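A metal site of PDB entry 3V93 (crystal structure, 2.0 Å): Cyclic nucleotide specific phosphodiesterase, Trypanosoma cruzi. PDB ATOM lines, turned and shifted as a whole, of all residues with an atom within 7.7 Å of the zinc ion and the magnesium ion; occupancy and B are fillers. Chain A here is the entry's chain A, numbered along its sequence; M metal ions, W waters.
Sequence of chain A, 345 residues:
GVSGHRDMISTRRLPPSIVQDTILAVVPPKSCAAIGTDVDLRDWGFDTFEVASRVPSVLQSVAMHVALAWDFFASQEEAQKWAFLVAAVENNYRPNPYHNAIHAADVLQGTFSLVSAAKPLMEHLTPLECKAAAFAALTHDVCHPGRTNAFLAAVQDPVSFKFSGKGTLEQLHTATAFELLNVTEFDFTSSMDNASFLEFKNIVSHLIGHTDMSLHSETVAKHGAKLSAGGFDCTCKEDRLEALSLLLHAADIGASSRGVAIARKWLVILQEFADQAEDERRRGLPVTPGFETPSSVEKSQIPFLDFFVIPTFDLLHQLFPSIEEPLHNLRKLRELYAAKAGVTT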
ATOM      1  N   TYR A  93       9.479 -13.612  12.287  1.00  0.00           N
ATOM      2  CA  TYR A  93      10.097 -13.918  10.995  1.00  0.00           C
ATOM      3  C   TYR A  93      11.149 -12.835  10.778  1.00  0.00           C
ATOM      4  O   TYR A  93      10.892 -11.671  11.037  1.00  0.00           O
ATOM      5  CB  TYR A  93       9.072 -13.862   9.850  1.00  0.00           C
ATOM      6  CG  TYR A  93       8.388 -15.189   9.583  1.00  0.00           C
ATOM      7  CD1 TYR A  93       8.977 -16.138   8.743  1.00  0.00           C
ATOM      8  CD2 TYR A  93       7.175 -15.507  10.193  1.00  0.00           C
ATOM      9  CE1 TYR A  93       8.373 -17.374   8.506  1.00  0.00           C
ATOM     10  CE2 TYR A  93       6.552 -16.744   9.970  1.00  0.00           C
ATOM     11  CZ  TYR A  93       7.157 -17.664   9.131  1.00  0.00           C
ATOM     12  OH  TYR A  93       6.554 -18.885   8.920  1.00  0.00           O
ATOM     13  N   TYR A  98      13.979 -14.036   1.178  1.00  0.00           N
ATOM     14  CA  TYR A  98      12.997 -15.086   0.860  1.00  0.00           C
ATOM     15  C   TYR A  98      12.251 -15.711   2.052  1.00  0.00           C
ATOM     16  O   TYR A  98      11.029 -15.687   2.090  1.00  0.00           O
ATOM     17  CB  TYR A  98      13.686 -16.216   0.077  1.00  0.00           C
ATOM     18  CG  TYR A  98      12.754 -17.337  -0.373  1.00  0.00           C
ATOM     19  CD1 TYR A  98      12.276 -17.414  -1.682  1.00  0.00           C
ATOM     20  CD2 TYR A  98      12.353 -18.332   0.530  1.00  0.00           C
ATOM     21  CE1 TYR A  98      11.427 -18.457  -2.091  1.00  0.00           C
ATOM     22  CE2 TYR A  98      11.500 -19.366   0.132  1.00  0.00           C
ATOM     23  CZ  TYR A  98      11.046 -19.426  -1.173  1.00  0.00           C
ATOM     24  OH  TYR A  98      10.220 -20.465  -1.559  1.00  0.00           O
ATOM     25  N   HIS A  99      12.981 -16.280   3.007  1.00  0.00           N
ATOM     26  CA  HIS A  99      12.320 -16.894   4.165  1.00  0.00           C
ATOM     27  C   HIS A  99      11.881 -15.845   5.172  1.00  0.00           C
ATOM     28  O   HIS A  99      12.478 -15.661   6.241  1.00  0.00           O
ATOM     29  CB  HIS A  99      13.248 -17.939   4.798  1.00  0.00           C
ATOM     30  CG  HIS A  99      13.597 -19.079   3.879  1.00  0.00           C
ATOM     31  ND1 HIS A  99      14.769 -19.126   3.160  1.00  0.00           N
ATOM     32  CD2 HIS A  99      12.880 -20.170   3.506  1.00  0.00           C
ATOM     33  CE1 HIS A  99      14.773 -20.195   2.383  1.00  0.00           C
ATOM     34  NE2 HIS A  99      13.639 -20.848   2.567  1.00  0.00           N
ATOM     35  N   ASN A 100      10.788 -15.165   4.808  1.00  0.00           N
ATOM     36  CA  ASN A 100      10.221 -14.090   5.621  1.00  0.00           C
ATOM     37  C   ASN A 100       8.708 -14.218   5.772  1.00  0.00           C
ATOM     38  O   ASN A 100       8.113 -15.201   5.319  1.00  0.00           O
ATOM     39  CB  ASN A 100      10.525 -12.753   4.945  1.00  0.00           C
ATOM     40  CG  ASN A 100      10.084 -12.726   3.501  1.00  0.00           C
ATOM     41  OD1 ASN A 100       8.945 -13.082   3.185  1.00  0.00           O
ATOM     42  ND2 ASN A 100      10.972 -12.319   2.595  1.00  0.00           N
ATOM     43  N   HIS A 103       6.738 -14.858   2.555  1.00  0.00           N
ATOM     44  CA  HIS A 103       6.781 -16.283   2.139  1.00  0.00           C
ATOM     45  C   HIS A 103       5.768 -17.036   2.977  1.00  0.00           C
ATOM     46  O   HIS A 103       5.039 -17.887   2.476  1.00  0.00           O
ATOM     47  CB  HIS A 103       8.187 -16.871   2.369  1.00  0.00           C
ATOM     48  CG  HIS A 103       8.273 -18.368   2.212  1.00  0.00           C
ATOM     49  ND1 HIS A 103       8.026 -19.015   1.023  1.00  0.00           N
ATOM     50  CD2 HIS A 103       8.650 -19.335   3.090  1.00  0.00           C
ATOM     51  CE1 HIS A 103       8.244 -20.315   1.176  1.00  0.00           C
ATOM     52  NE2 HIS A 103       8.627 -20.533   2.416  1.00  0.00           N
ATOM     53  N   ALA A 104       5.706 -16.732   4.276  1.00  0.00           N
ATOM     54  CA  ALA A 104       4.764 -17.388   5.163  1.00  0.00           C
ATOM     55  C   ALA A 104       3.347 -17.149   4.673  1.00  0.00           C
ATOM     56  O   ALA A 104       2.547 -18.080   4.576  1.00  0.00           O
ATOM     57  CB  ALA A 104       4.917 -16.871   6.601  1.00  0.00           C
ATOM     58  N   VAL A 107       2.687 -19.160   1.498  1.00  0.00           N
ATOM     59  CA  VAL A 107       2.490 -20.585   1.729  1.00  0.00           C
ATOM     60  C   VAL A 107       1.134 -20.829   2.382  1.00  0.00           C
ATOM     61  O   VAL A 107       0.457 -21.813   2.078  1.00  0.00           O
ATOM     62  CB  VAL A 107       3.634 -21.167   2.585  1.00  0.00           C
ATOM     63  CG1 VAL A 107       3.389 -22.655   2.895  1.00  0.00           C
ATOM     64  CG2 VAL A 107       4.949 -21.022   1.819  1.00  0.00           C
ATOM     65  N   ALA A 137       1.176 -23.800   8.137  1.00  0.00           N
ATOM     66  CA  ALA A 137       1.647 -23.020   6.988  1.00  0.00           C
ATOM     67  C   ALA A 137       2.148 -21.657   7.463  1.00  0.00           C
ATOM     68  O   ALA A 137       3.197 -21.189   7.041  1.00  0.00           O
ATOM     69  CB  ALA A 137       0.517 -22.831   5.992  1.00  0.00           C
ATOM     70  N   HIS A 140       5.450 -22.323   9.426  1.00  0.00           N
ATOM     71  CA  HIS A 140       6.411 -23.297   8.903  1.00  0.00           C
ATOM     72  C   HIS A 140       7.886 -22.897   8.784  1.00  0.00           C
ATOM     73  O   HIS A 140       8.747 -23.769   8.791  1.00  0.00           O
ATOM     74  CB  HIS A 140       5.932 -23.879   7.564  1.00  0.00           C
ATOM     75  CG  HIS A 140       6.404 -23.129   6.355  1.00  0.00           C
ATOM     76  ND1 HIS A 140       5.793 -21.971   5.919  1.00  0.00           N
ATOM     77  CD2 HIS A 140       7.445 -23.348   5.522  1.00  0.00           C
ATOM     78  CE1 HIS A 140       6.449 -21.507   4.860  1.00  0.00           C
ATOM     79  NE2 HIS A 140       7.457 -22.320   4.599  1.00  0.00           N
ATOM     80  N   ASP A 141       8.171 -21.594   8.680  1.00  0.00           N
ATOM     81  CA  ASP A 141       9.549 -21.104   8.561  1.00  0.00           C
ATOM     82  C   ASP A 141       9.877 -20.056   9.646  1.00  0.00           C
ATOM     83  O   ASP A 141      10.860 -19.332   9.522  1.00  0.00           O
ATOM     84  CB  ASP A 141       9.785 -20.466   7.173  1.00  0.00           C
ATOM     85  CG  ASP A 141      10.241 -21.468   6.124  1.00  0.00           C
ATOM     86  OD1 ASP A 141      10.853 -22.474   6.516  1.00  0.00           O
ATOM     87  OD2 ASP A 141      10.011 -21.246   4.915  1.00  0.00           O
ATOM     88  N   VAL A 142       9.076 -19.988  10.700  1.00  0.00           N
ATOM     89  CA  VAL A 142       9.305 -18.995  11.739  1.00  0.00           C
ATOM     90  C   VAL A 142      10.716 -19.044  12.310  1.00  0.00           C
ATOM     91  O   VAL A 142      11.245 -20.120  12.617  1.00  0.00           O
ATOM     92  CB  VAL A 142       8.251 -19.109  12.887  1.00  0.00           C
ATOM     93  CG1 VAL A 142       8.446 -20.394  13.684  1.00  0.00           C
ATOM     94  CG2 VAL A 142       8.311 -17.871  13.778  1.00  0.00           C
ATOM     95  N   HIS A 144      13.418 -18.483  10.720  1.00  0.00           N
ATOM     96  CA  HIS A 144      14.386 -18.932   9.726  1.00  0.00           C
ATOM     97  C   HIS A 144      15.505 -17.874   9.618  1.00  0.00           C
ATOM     98  O   HIS A 144      15.238 -16.688   9.435  1.00  0.00           O
ATOM     99  CB  HIS A 144      13.697 -19.128   8.373  1.00  0.00           C
ATOM    100  CG  HIS A 144      14.476 -19.966   7.408  1.00  0.00           C
ATOM    101  ND1 HIS A 144      15.727 -19.597   6.948  1.00  0.00           N
ATOM    102  CD2 HIS A 144      14.174 -21.134   6.792  1.00  0.00           C
ATOM    103  CE1 HIS A 144      16.166 -20.514   6.107  1.00  0.00           C
ATOM    104  NE2 HIS A 144      15.240 -21.453   5.990  1.00  0.00           N
ATOM    105  N   ASN A 149      20.152 -25.863   6.542  1.00  0.00           N
ATOM    106  CA  ASN A 149      20.449 -26.800   7.622  1.00  0.00           C
ATOM    107  C   ASN A 149      21.935 -27.188   7.515  1.00  0.00           C
ATOM    108  O   ASN A 149      22.619 -27.345   8.520  1.00  0.00           O
ATOM    109  CB  ASN A 149      19.606 -28.080   7.496  1.00  0.00           C
ATOM    110  CG  ASN A 149      18.172 -27.877   7.973  1.00  0.00           C
ATOM    111  OD1 ASN A 149      17.909 -27.086   8.872  1.00  0.00           O
ATOM    112  ND2 ASN A 149      17.233 -28.620   7.361  1.00  0.00           N
ATOM    113  N   LEU A 169      16.192 -27.059  11.064  1.00  0.00           N
ATOM    114  CA  LEU A 169      15.355 -25.873  11.116  1.00  0.00           C
ATOM    115  C   LEU A 169      13.870 -26.220  11.226  1.00  0.00           C
ATOM    116  O   LEU A 169      13.124 -25.543  11.947  1.00  0.00           O
ATOM    117  CB  LEU A 169      15.580 -24.987   9.883  1.00  0.00           C
ATOM    118  CG  LEU A 169      16.850 -24.124   9.934  1.00  0.00           C
ATOM    119  CD1 LEU A 169      17.048 -23.402   8.607  1.00  0.00           C
ATOM    120  CD2 LEU A 169      16.741 -23.124  11.076  1.00  0.00           C
ATOM    121  N   GLU A 170      13.455 -27.260  10.516  1.00  0.00           N
ATOM    122  CA  GLU A 170      12.067 -27.674  10.563  1.00  0.00           C
ATOM    123  C   GLU A 170      11.634 -28.001  12.001  1.00  0.00           C
ATOM    124  O   GLU A 170      10.539 -27.622  12.436  1.00  0.00           O
ATOM    125  CB  GLU A 170      11.852 -28.863   9.637  1.00  0.00           C
ATOM    126  CG  GLU A 170      11.965 -28.542   8.141  1.00  0.00           C
ATOM    127  CD  GLU A 170      13.384 -28.214   7.668  1.00  0.00           C
ATOM    128  OE1 GLU A 170      14.363 -28.661   8.303  1.00  0.00           O
ATOM    129  OE2 GLU A 170      13.514 -27.522   6.641  1.00  0.00           O
ATOM    130  N   HIS A 173      11.357 -24.660  13.835  1.00  0.00           N
ATOM    131  CA  HIS A 173      10.144 -23.912  13.489  1.00  0.00           C
ATOM    132  C   HIS A 173       8.971 -24.510  14.270  1.00  0.00           C
ATOM    133  O   HIS A 173       8.137 -23.788  14.841  1.00  0.00           O
ATOM    134  CB  HIS A 173       9.829 -23.985  11.980  1.00  0.00           C
ATOM    135  CG  HIS A 173      10.942 -23.507  11.095  1.00  0.00           C
ATOM    136  ND1 HIS A 173      11.618 -22.321  11.304  1.00  0.00           N
ATOM    137  CD2 HIS A 173      11.492 -24.055   9.981  1.00  0.00           C
ATOM    138  CE1 HIS A 173      12.537 -22.165  10.365  1.00  0.00           C
ATOM    139  NE2 HIS A 173      12.483 -23.203   9.553  1.00  0.00           N
ATOM    140  N   ILE A 208       4.816 -29.413   9.308  1.00  0.00           N
ATOM    141  CA  ILE A 208       6.018 -28.590   9.274  1.00  0.00           C
ATOM    142  C   ILE A 208       7.227 -29.483   9.033  1.00  0.00           C
ATOM    143  O   ILE A 208       8.147 -29.111   8.307  1.00  0.00           O
ATOM    144  CB  ILE A 208       6.202 -27.799  10.598  1.00  0.00           C
ATOM    145  CG1 ILE A 208       5.032 -26.837  10.779  1.00  0.00           C
ATOM    146  CG2 ILE A 208       7.534 -27.039  10.575  1.00  0.00           C
ATOM    147  CD1 ILE A 208       5.166 -25.897  11.977  1.00  0.00           C
ATOM    148  N   THR A 211       8.229 -30.230   5.409  1.00  0.00           N
ATOM    149  CA  THR A 211       8.628 -29.146   4.518  1.00  0.00           C
ATOM    150  C   THR A 211      10.137 -29.243   4.320  1.00  0.00           C
ATOM    151  O   THR A 211      10.724 -28.497   3.528  1.00  0.00           O
ATOM    152  CB  THR A 211       8.281 -27.748   5.094  1.00  0.00           C
ATOM    153  OG1 THR A 211       8.913 -27.574   6.370  1.00  0.00           O
ATOM    154  CG2 THR A 211       6.757 -27.590   5.249  1.00  0.00           C
ATOM    155  N   ASP A 212      10.751 -30.178   5.039  1.00  0.00           N
ATOM    156  CA  ASP A 212      12.194 -30.420   4.933  1.00  0.00           C
ATOM    157  C   ASP A 212      12.509 -30.917   3.528  1.00  0.00           C
ATOM    158  O   ASP A 212      12.075 -31.993   3.130  1.00  0.00           O
ATOM    159  CB  ASP A 212      12.648 -31.470   5.950  1.00  0.00           C
ATOM    160  CG  ASP A 212      14.099 -31.881   5.766  1.00  0.00           C
ATOM    161  OD1 ASP A 212      14.514 -32.915   6.327  1.00  0.00           O
ATOM    162  OD2 ASP A 212      14.843 -31.154   5.061  1.00  0.00           O
ATOM    163  N   MET A 213      13.279 -30.133   2.788  1.00  0.00           N
ATOM    164  CA  MET A 213      13.622 -30.506   1.416  1.00  0.00           C
ATOM    165  C   MET A 213      14.335 -31.838   1.269  1.00  0.00           C
ATOM    166  O   MET A 213      14.327 -32.421   0.187  1.00  0.00           O
ATOM    167  CB  MET A 213      14.465 -29.409   0.771  1.00  0.00           C
ATOM    168  CG  MET A 213      13.662 -28.191   0.360  1.00  0.00           C
ATOM    169  SD  MET A 213      12.197 -28.683  -0.566  1.00  0.00           S
ATOM    170  CE  MET A 213      12.920 -29.079  -2.181  1.00  0.00           C
ATOM    171  N   LEU A 248       0.888 -28.794   1.380  1.00  0.00           N
ATOM    172  CA  LEU A 248       1.635 -27.742   2.055  1.00  0.00           C
ATOM    173  C   LEU A 248       3.026 -27.641   1.444  1.00  0.00           C
ATOM    174  O   LEU A 248       3.540 -26.541   1.187  1.00  0.00           O
ATOM    175  CB  LEU A 248       1.771 -28.031   3.556  1.00  0.00           C
ATOM    176  CG  LEU A 248       2.878 -27.212   4.241  1.00  0.00           C
ATOM    177  CD1 LEU A 248       2.534 -25.742   4.152  1.00  0.00           C
ATOM    178  CD2 LEU A 248       3.022 -27.638   5.703  1.00  0.00           C
ATOM    179  N   HIS A 249       3.643 -28.790   1.231  1.00  0.00           N
ATOM    180  CA  HIS A 249       4.969 -28.850   0.632  1.00  0.00           C
ATOM    181  C   HIS A 249       4.953 -28.221  -0.770  1.00  0.00           C
ATOM    182  O   HIS A 249       5.850 -27.448  -1.122  1.00  0.00           O
ATOM    183  CB  HIS A 249       5.432 -30.307   0.545  1.00  0.00           C
ATOM    184  CG  HIS A 249       6.704 -30.504  -0.226  1.00  0.00           C
ATOM    185  ND1 HIS A 249       7.867 -29.819   0.060  1.00  0.00           N
ATOM    186  CD2 HIS A 249       7.003 -31.324  -1.258  1.00  0.00           C
ATOM    187  CE1 HIS A 249       8.828 -30.208  -0.758  1.00  0.00           C
ATOM    188  NE2 HIS A 249       8.326 -31.131  -1.574  1.00  0.00           N
ATOM    189  N   ALA A 251       2.876 -26.021  -1.884  1.00  0.00           N
ATOM    190  CA  ALA A 251       2.660 -24.584  -1.733  1.00  0.00           C
ATOM    191  C   ALA A 251       3.975 -23.922  -1.329  1.00  0.00           C
ATOM    192  O   ALA A 251       4.305 -22.831  -1.791  1.00  0.00           O
ATOM    193  CB  ALA A 251       1.591 -24.316  -0.659  1.00  0.00           C
ATOM    194  N   ASP A 252       4.732 -24.589  -0.465  1.00  0.00           N
ATOM    195  CA  ASP A 252       6.024 -24.085   0.028  1.00  0.00           C
ATOM    196  C   ASP A 252       7.015 -23.855  -1.112  1.00  0.00           C
ATOM    197  O   ASP A 252       7.646 -22.799  -1.182  1.00  0.00           O
ATOM    198  CB  ASP A 252       6.584 -25.092   1.048  1.00  0.00           C
ATOM    199  CG  ASP A 252       7.777 -24.538   1.860  1.00  0.00           C
ATOM    200  OD1 ASP A 252       7.985 -23.302   1.989  1.00  0.00           O
ATOM    201  OD2 ASP A 252       8.510 -25.397   2.401  1.00  0.00           O
ATOM    202  N   ILE A 253       7.153 -24.829  -2.022  1.00  0.00           N
ATOM    203  CA  ILE A 253       8.101 -24.704  -3.131  1.00  0.00           C
ATOM    204  C   ILE A 253       7.478 -24.307  -4.465  1.00  0.00           C
ATOM    205  O   ILE A 253       8.177 -24.254  -5.472  1.00  0.00           O
ATOM    206  CB  ILE A 253       8.838 -26.045  -3.403  1.00  0.00           C
ATOM    207  CG1 ILE A 253       7.872 -27.036  -4.043  1.00  0.00           C
ATOM    208  CG2 ILE A 253       9.399 -26.613  -2.115  1.00  0.00           C
ATOM    209  CD1 ILE A 253       8.524 -28.337  -4.498  1.00  0.00           C
HETATM  210 ZN    ZN M   1       9.174 -22.335   3.379  1.00  0.00          ZN
HETATM  211 MG    MG M   2      11.366 -24.273   5.614  1.00  0.00          MG
HETATM  212  O   HOH W   1      12.905 -23.399   4.132  1.00  0.00           O
HETATM  213  O   HOH W   2      12.005 -26.438   4.934  1.00  0.00           O
HETATM  214  O   HOH W   3      10.040 -25.256   7.106  1.00  0.00           O
HETATM  215  O   HOH W   4      13.160 -24.442   7.057  1.00  0.00           O
HETATM  216  O   HOH W   5       9.862 -24.209   4.018  1.00  0.00           O
HETATM  217  O   HOH W   6      11.127 -22.390   1.954  1.00  0.00           O
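N of Asp 141 lies within hydrogen-bond range of OH of Tyr 93, 3.2 Å away.
O of Asp 252 lies within hydrogen-bond range of OH of Tyr 98.
ND1 of His 140 sits at hydrogen-bond distance from O of Ala 137 (2.9 Å).
N of His 103 lies within hydrogen-bond range of OD1 of Asn 100 (2.9 Å).
Of the 25 residues printed, 4 come within 4 Å of the zinc ion.
One residue has an atom within 4 Å of the magnesium ion: Asp 141.
The zinc ion is bound by the side-chain carboxylate of Asp 141 (2.1 Å), the side-chain carboxylate of Asp 252 (2.1 Å), water W5 (2.1 Å), a ring nitrogen (NE2) of His 140 (2.1 Å), a ring nitrogen (NE2) of His 103 (2.1 Å) and water W6 (2.4 Å).
The magnesium ion is bound by OD1 of Asp 141 (2.1 Å), water W5 (2.2 Å), water W3 (2.2 Å), water W1 (2.3 Å), water W4 (2.3 Å) and water W2 (2.4 Å).
The magnesium ion has six donor atoms within binding distance.
Water W4 bridges NE2 of His 173 and OE2 of Glu 170.
Water W2 bridges OE2 of Glu 170 (2.5 Å) and O of Thr 211 (2.8 Å).
Water W3 lies within hydrogen-bond range of O of His 140 (2.6 Å) and OG1 of Thr 211 (2.7 Å).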
